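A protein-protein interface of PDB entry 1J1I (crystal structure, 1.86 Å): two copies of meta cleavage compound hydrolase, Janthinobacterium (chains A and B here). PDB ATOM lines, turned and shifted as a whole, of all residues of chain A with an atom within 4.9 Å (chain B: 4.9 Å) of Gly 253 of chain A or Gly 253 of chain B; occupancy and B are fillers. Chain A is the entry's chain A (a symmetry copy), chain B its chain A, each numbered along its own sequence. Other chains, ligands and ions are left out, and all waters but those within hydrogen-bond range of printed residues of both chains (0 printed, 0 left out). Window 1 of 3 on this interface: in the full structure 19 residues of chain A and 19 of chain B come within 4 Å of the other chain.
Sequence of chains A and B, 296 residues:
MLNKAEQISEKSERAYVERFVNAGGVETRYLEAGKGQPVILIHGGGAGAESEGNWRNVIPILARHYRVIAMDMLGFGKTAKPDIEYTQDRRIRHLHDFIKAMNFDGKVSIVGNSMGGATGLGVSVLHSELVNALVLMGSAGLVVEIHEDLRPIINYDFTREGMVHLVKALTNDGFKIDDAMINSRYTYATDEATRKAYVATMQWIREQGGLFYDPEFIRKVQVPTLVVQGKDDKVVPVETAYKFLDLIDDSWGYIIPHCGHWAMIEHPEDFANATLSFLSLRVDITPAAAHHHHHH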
ATOM      1  N   LEU A 226      -0.305 -27.691  28.993  1.00  0.00           N
ATOM      2  CA  LEU A 226      -1.642 -27.369  28.506  1.00  0.00           C
ATOM      3  C   LEU A 226      -2.114 -28.608  27.747  1.00  0.00           C
ATOM      4  O   LEU A 226      -1.507 -28.999  26.749  1.00  0.00           O
ATOM      5  CB  LEU A 226      -1.596 -26.173  27.550  1.00  0.00           C
ATOM      6  CG  LEU A 226      -2.812 -25.244  27.414  1.00  0.00           C
ATOM      7  CD1 LEU A 226      -2.984 -24.855  25.949  1.00  0.00           C
ATOM      8  CD2 LEU A 226      -4.064 -25.905  27.939  1.00  0.00           C
ATOM      9  N   VAL A 227      -3.173 -29.242  28.240  1.00  0.00           N
ATOM     10  CA  VAL A 227      -3.726 -30.424  27.587  1.00  0.00           C
ATOM     11  C   VAL A 227      -4.890 -29.935  26.723  1.00  0.00           C
ATOM     12  O   VAL A 227      -5.920 -29.504  27.249  1.00  0.00           O
ATOM     13  CB  VAL A 227      -4.248 -31.457  28.622  1.00  0.00           C
ATOM     14  CG1 VAL A 227      -4.803 -32.682  27.912  1.00  0.00           C
ATOM     15  CG2 VAL A 227      -3.120 -31.864  29.570  1.00  0.00           C
ATOM     16  N   LEU A 245      -4.986 -34.597  33.010  1.00  0.00           N
ATOM     17  CA  LEU A 245      -5.171 -33.520  33.979  1.00  0.00           C
ATOM     18  C   LEU A 245      -5.013 -34.003  35.416  1.00  0.00           C
ATOM     19  O   LEU A 245      -4.580 -33.254  36.287  1.00  0.00           O
ATOM     20  CB  LEU A 245      -6.544 -32.860  33.772  1.00  0.00           C
ATOM     21  CG  LEU A 245      -6.660 -32.038  32.478  1.00  0.00           C
ATOM     22  CD1 LEU A 245      -8.090 -31.540  32.295  1.00  0.00           C
ATOM     23  CD2 LEU A 245      -5.699 -30.857  32.534  1.00  0.00           C
ATOM     24  N   SER A 251      -0.799 -29.015  35.128  1.00  0.00           N
ATOM     25  CA  SER A 251      -1.486 -28.999  33.845  1.00  0.00           C
ATOM     26  C   SER A 251      -2.814 -28.249  33.833  1.00  0.00           C
ATOM     27  O   SER A 251      -3.615 -28.341  34.765  1.00  0.00           O
ATOM     28  CB  SER A 251      -1.720 -30.428  33.341  1.00  0.00           C
ATOM     29  OG  SER A 251      -2.576 -31.166  34.200  1.00  0.00           O
ATOM     30  N   TRP A 252      -3.007 -27.495  32.756  1.00  0.00           N
ATOM     31  CA  TRP A 252      -4.222 -26.733  32.499  1.00  0.00           C
ATOM     32  C   TRP A 252      -4.929 -27.558  31.436  1.00  0.00           C
ATOM     33  O   TRP A 252      -4.287 -28.337  30.729  1.00  0.00           O
ATOM     34  CB  TRP A 252      -3.883 -25.367  31.910  1.00  0.00           C
ATOM     35  CG  TRP A 252      -3.557 -24.291  32.895  1.00  0.00           C
ATOM     36  CD1 TRP A 252      -4.368 -23.257  33.275  1.00  0.00           C
ATOM     37  CD2 TRP A 252      -2.315 -24.102  33.590  1.00  0.00           C
ATOM     38  NE1 TRP A 252      -3.708 -22.432  34.152  1.00  0.00           N
ATOM     39  CE2 TRP A 252      -2.444 -22.924  34.363  1.00  0.00           C
ATOM     40  CE3 TRP A 252      -1.101 -24.808  33.626  1.00  0.00           C
ATOM     41  CZ2 TRP A 252      -1.413 -22.440  35.173  1.00  0.00           C
ATOM     42  CZ3 TRP A 252      -0.070 -24.325  34.433  1.00  0.00           C
ATOM     43  CH2 TRP A 252      -0.233 -23.149  35.191  1.00  0.00           C
ATOM     44  N   GLY A 253      -6.242 -27.394  31.316  1.00  0.00           N
ATOM     45  CA  GLY A 253      -6.970 -28.140  30.310  1.00  0.00           C
ATOM     46  C   GLY A 253      -7.768 -27.211  29.417  1.00  0.00           C
ATOM     47  O   GLY A 253      -8.304 -26.204  29.892  1.00  0.00           O
ATOM     48  N   TYR A 254      -7.816 -27.526  28.124  1.00  0.00           N
ATOM     49  CA  TYR A 254      -8.586 -26.741  27.155  1.00  0.00           C
ATOM     50  C   TYR A 254      -9.356 -27.729  26.289  1.00  0.00           C
ATOM     51  O   TYR A 254      -8.784 -28.406  25.427  1.00  0.00           O
ATOM     52  CB  TYR A 254      -7.681 -25.873  26.276  1.00  0.00           C
ATOM     53  CG  TYR A 254      -8.450 -24.899  25.401  1.00  0.00           C
ATOM     54  CD1 TYR A 254      -9.328 -23.975  25.966  1.00  0.00           C
ATOM     55  CD2 TYR A 254      -8.319 -24.916  24.010  1.00  0.00           C
ATOM     56  CE1 TYR A 254     -10.059 -23.094  25.178  1.00  0.00           C
ATOM     57  CE2 TYR A 254      -9.047 -24.035  23.208  1.00  0.00           C
ATOM     58  CZ  TYR A 254      -9.919 -23.128  23.804  1.00  0.00           C
ATOM     59  OH  TYR A 254     -10.666 -22.271  23.032  1.00  0.00           O
ATOM     60  N   ILE A 255     -10.663 -27.799  26.526  1.00  0.00           N
ATOM     61  CA  ILE A 255     -11.535 -28.722  25.815  1.00  0.00           C
ATOM     62  C   ILE A 255     -12.314 -27.965  24.750  1.00  0.00           C
ATOM     63  O   ILE A 255     -12.963 -26.955  25.039  1.00  0.00           O
ATOM     64  CB  ILE A 255     -12.503 -29.401  26.800  1.00  0.00           C
ATOM     65  CG1 ILE A 255     -11.739 -29.851  28.056  1.00  0.00           C
ATOM     66  CG2 ILE A 255     -13.171 -30.589  26.139  1.00  0.00           C
ATOM     67  CD1 ILE A 255     -10.673 -30.906  27.814  1.00  0.00           C
ATOM     68  N   LEU B 226     -18.083 -21.131  27.860  1.00  0.00           N
ATOM     69  CA  LEU B 226     -16.750 -21.460  28.350  1.00  0.00           C
ATOM     70  C   LEU B 226     -16.941 -21.900  29.801  1.00  0.00           C
ATOM     71  O   LEU B 226     -17.392 -21.116  30.637  1.00  0.00           O
ATOM     72  CB  LEU B 226     -15.837 -20.231  28.306  1.00  0.00           C
ATOM     73  CG  LEU B 226     -14.320 -20.400  28.129  1.00  0.00           C
ATOM     74  CD1 LEU B 226     -13.597 -19.393  29.018  1.00  0.00           C
ATOM     75  CD2 LEU B 226     -13.886 -21.808  28.457  1.00  0.00           C
ATOM     76  N   VAL B 227     -16.630 -23.159  30.089  1.00  0.00           N
ATOM     77  CA  VAL B 227     -16.752 -23.683  31.446  1.00  0.00           C
ATOM     78  C   VAL B 227     -15.359 -23.591  32.070  1.00  0.00           C
ATOM     79  O   VAL B 227     -14.443 -24.314  31.664  1.00  0.00           O
ATOM     80  CB  VAL B 227     -17.223 -25.162  31.448  1.00  0.00           C
ATOM     81  CG1 VAL B 227     -17.354 -25.674  32.873  1.00  0.00           C
ATOM     82  CG2 VAL B 227     -18.561 -25.286  30.717  1.00  0.00           C
ATOM     83  N   LEU B 245     -19.609 -29.926  30.318  1.00  0.00           N
ATOM     84  CA  LEU B 245     -19.065 -30.091  28.973  1.00  0.00           C
ATOM     85  C   LEU B 245     -19.827 -31.136  28.166  1.00  0.00           C
ATOM     86  O   LEU B 245     -19.924 -31.040  26.946  1.00  0.00           O
ATOM     87  CB  LEU B 245     -17.570 -30.446  29.054  1.00  0.00           C
ATOM     88  CG  LEU B 245     -16.674 -29.294  29.533  1.00  0.00           C
ATOM     89  CD1 LEU B 245     -15.238 -29.779  29.712  1.00  0.00           C
ATOM     90  CD2 LEU B 245     -16.718 -28.155  28.522  1.00  0.00           C
ATOM     91  N   SER B 251     -20.003 -25.912  24.243  1.00  0.00           N
ATOM     92  CA  SER B 251     -19.152 -25.515  25.356  1.00  0.00           C
ATOM     93  C   SER B 251     -17.688 -25.919  25.224  1.00  0.00           C
ATOM     94  O   SER B 251     -17.360 -27.022  24.786  1.00  0.00           O
ATOM     95  CB  SER B 251     -19.703 -26.067  26.676  1.00  0.00           C
ATOM     96  OG  SER B 251     -19.700 -27.487  26.707  1.00  0.00           O
ATOM     97  N   TRP B 252     -16.827 -24.981  25.604  1.00  0.00           N
ATOM     98  CA  TRP B 252     -15.379 -25.159  25.620  1.00  0.00           C
ATOM     99  C   TRP B 252     -15.069 -25.338  27.097  1.00  0.00           C
ATOM    100  O   TRP B 252     -15.851 -24.912  27.950  1.00  0.00           O
ATOM    101  CB  TRP B 252     -14.680 -23.897  25.126  1.00  0.00           C
ATOM    102  CG  TRP B 252     -14.530 -23.768  23.643  1.00  0.00           C
ATOM    103  CD1 TRP B 252     -13.387 -23.962  22.918  1.00  0.00           C
ATOM    104  CD2 TRP B 252     -15.537 -23.364  22.705  1.00  0.00           C
ATOM    105  NE1 TRP B 252     -13.614 -23.696  21.591  1.00  0.00           N
ATOM    106  CE2 TRP B 252     -14.926 -23.323  21.429  1.00  0.00           C
ATOM    107  CE3 TRP B 252     -16.895 -23.021  22.818  1.00  0.00           C
ATOM    108  CZ2 TRP B 252     -15.625 -22.966  20.272  1.00  0.00           C
ATOM    109  CZ3 TRP B 252     -17.594 -22.663  21.663  1.00  0.00           C
ATOM    110  CH2 TRP B 252     -16.954 -22.634  20.408  1.00  0.00           C
ATOM    111  N   GLY B 253     -13.938 -25.963  27.408  1.00  0.00           N
ATOM    112  CA  GLY B 253     -13.581 -26.150  28.798  1.00  0.00           C
ATOM    113  C   GLY B 253     -12.196 -25.598  29.081  1.00  0.00           C
ATOM    114  O   GLY B 253     -11.304 -25.702  28.233  1.00  0.00           O
ATOM    115  N   TYR B 254     -12.030 -24.983  30.250  1.00  0.00           N
ATOM    116  CA  TYR B 254     -10.736 -24.441  30.671  1.00  0.00           C
ATOM    117  C   TYR B 254     -10.522 -24.863  32.120  1.00  0.00           C
ATOM    118  O   TYR B 254     -11.152 -24.331  33.041  1.00  0.00           O
ATOM    119  CB  TYR B 254     -10.693 -22.914  30.563  1.00  0.00           C
ATOM    120  CG  TYR B 254      -9.309 -22.334  30.797  1.00  0.00           C
ATOM    121  CD1 TYR B 254      -8.227 -22.739  30.018  1.00  0.00           C
ATOM    122  CD2 TYR B 254      -9.078 -21.400  31.810  1.00  0.00           C
ATOM    123  CE1 TYR B 254      -6.949 -22.238  30.236  1.00  0.00           C
ATOM    124  CE2 TYR B 254      -7.800 -20.887  32.037  1.00  0.00           C
ATOM    125  CZ  TYR B 254      -6.739 -21.317  31.245  1.00  0.00           C
ATOM    126  OH  TYR B 254      -5.467 -20.847  31.468  1.00  0.00           O
ATOM    127  N   ILE B 255      -9.625 -25.825  32.308  1.00  0.00           N
ATOM    128  CA  ILE B 255      -9.333 -26.372  33.625  1.00  0.00           C
ATOM    129  C   ILE B 255      -8.024 -25.790  34.137  1.00  0.00           C
ATOM    130  O   ILE B 255      -6.998 -25.843  33.453  1.00  0.00           O
ATOM    131  CB  ILE B 255      -9.239 -27.907  33.553  1.00  0.00           C
ATOM    132  CG1 ILE B 255     -10.401 -28.461  32.711  1.00  0.00           C
ATOM    133  CG2 ILE B 255      -9.275 -28.498  34.947  1.00  0.00           C
ATOM    134  CD1 ILE B 255     -11.785 -28.210  33.285  1.00  0.00           C
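O of Trp 252 of chain B lies within hydrogen-bond range of N of Val 227 of chain B, 2.9 Å away.
The backbone carbonyl oxygen of Val 227 of chain A is in hydrogen-bond range of the backbone NH of Tyr 254 of chain A, 2.9 Å away.
The backbone carbonyl oxygen (O) of Val 227 of chain B sits at hydrogen-bond distance from the backbone NH (N) of Tyr 254 of chain B.
The backbone NH of Val 227 of chain A sits at hydrogen-bond distance from the backbone carbonyl oxygen of Trp 252 of chain A, at 2.9 Å.
Printed residues of chain B within 4 Å of Leu 245 of chain A: Ile 255 (3.9 Å).
Ser 251 of chain A touches none of the printed residues of chain B.
Of chain B, only Gly 253, Tyr 254 and Ile 255 come within 4 Å of Gly 253 of chain A.
Printed residues of chain B within 4 Å of Tyr 254 of chain A: Trp 252 and Gly 253.
Printed residues of chain B within 4 Å of Ile 255 of chain A: Leu 245 (3.9 Å), Trp 252 (3.1 Å) and Gly 253 (2.7 Å).
Gly 253 of chain B touches just these residues of chain A: Gly 253 (3.5 Å), Tyr 254 (3.1 Å) and Ile 255 (2.7 Å).
Of the printed residues of chain A, Tyr 254 of chain B touches Trp 252 (3.2 Å) and Gly 253 (3.1 Å).
The nearest printed residue of chain B that does not touch Gly 253 of chain A is Val 227 of chain B (6.7 Å).
The nearest printed residue of chain A that does not touch Gly 253 of chain B is Val 227 of chain A (6.7 Å).
The nearest printed residue of chain B that does not touch Trp 252 of chain A is Gly 253 of chain B (7.4 Å).
Hydrophobic or aromatic side chains of chain A within 4 Å of the printed part of chain B: Leu 245, Trp 252, Tyr 254 and Ile 255.
Of the 8 printed residues of chain B, 5 touch a printed residue of chain A.
Hydrophobic or aromatic side chains of chain B that line the printed part of chain A: Leu 245, Trp 252, Tyr 254 and Ile 255.
Along chain B the printed residues that touch a printed residue of chain A span positions 245 to 255.
Among the printed residues, no Asp or Glu carboxylate lies within 4 Å of a Lys or Arg side-chain nitrogen of the other chain.
Leu 245 of chain A touches Ile 255 of chain B, and with the chains exchanged Ile 255 of chain A touches Leu 245 of chain B.
Trp 252 of chain A touches Tyr 254 of chain B, and with the chains exchanged Tyr 254 of chain A touches Trp 252 of chain B.
Gly 253 of chain A touches its own counterpart, Gly 253 of chain B.
Gly 253 of chain A touches Tyr 254 of chain B, and with the chains exchanged Tyr 254 of chain A touches Gly 253 of chain B.
O of Ile 255 of chain B lies within hydrogen-bond range of N of Gly 253 of chain A, at 2.7 Å.
O of Gly 253 of chain A sits close to O of Gly 253 of chain B, at 3.5 Å.
N of Gly 253 of chain B is in hydrogen-bond range of O of Ile 255 of chain A (2.7 Å).
Ile 255 of chain B touches Leu 245 of chain A (CG1 to CD1, 3.9 Å).
Trp 252 of chain A touches Tyr 254 of chain B.
CA of Trp 252 of chain A touches O of Ile 255 of chain B, at 3.1 Å.
O of Gly 253 of chain A touches CA of Tyr 254 of chain B, 3.1 Å away.
Trp 252 of chain B touches Tyr 254 of chain A.
Tyr 254 of chain A touches Gly 253 of chain B.
CG1 of Ile 255 of chain A touches CD1 of Leu 245 of chain B, 3.9 Å away.
Ile 255 of chain A touches Trp 252 of chain B.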
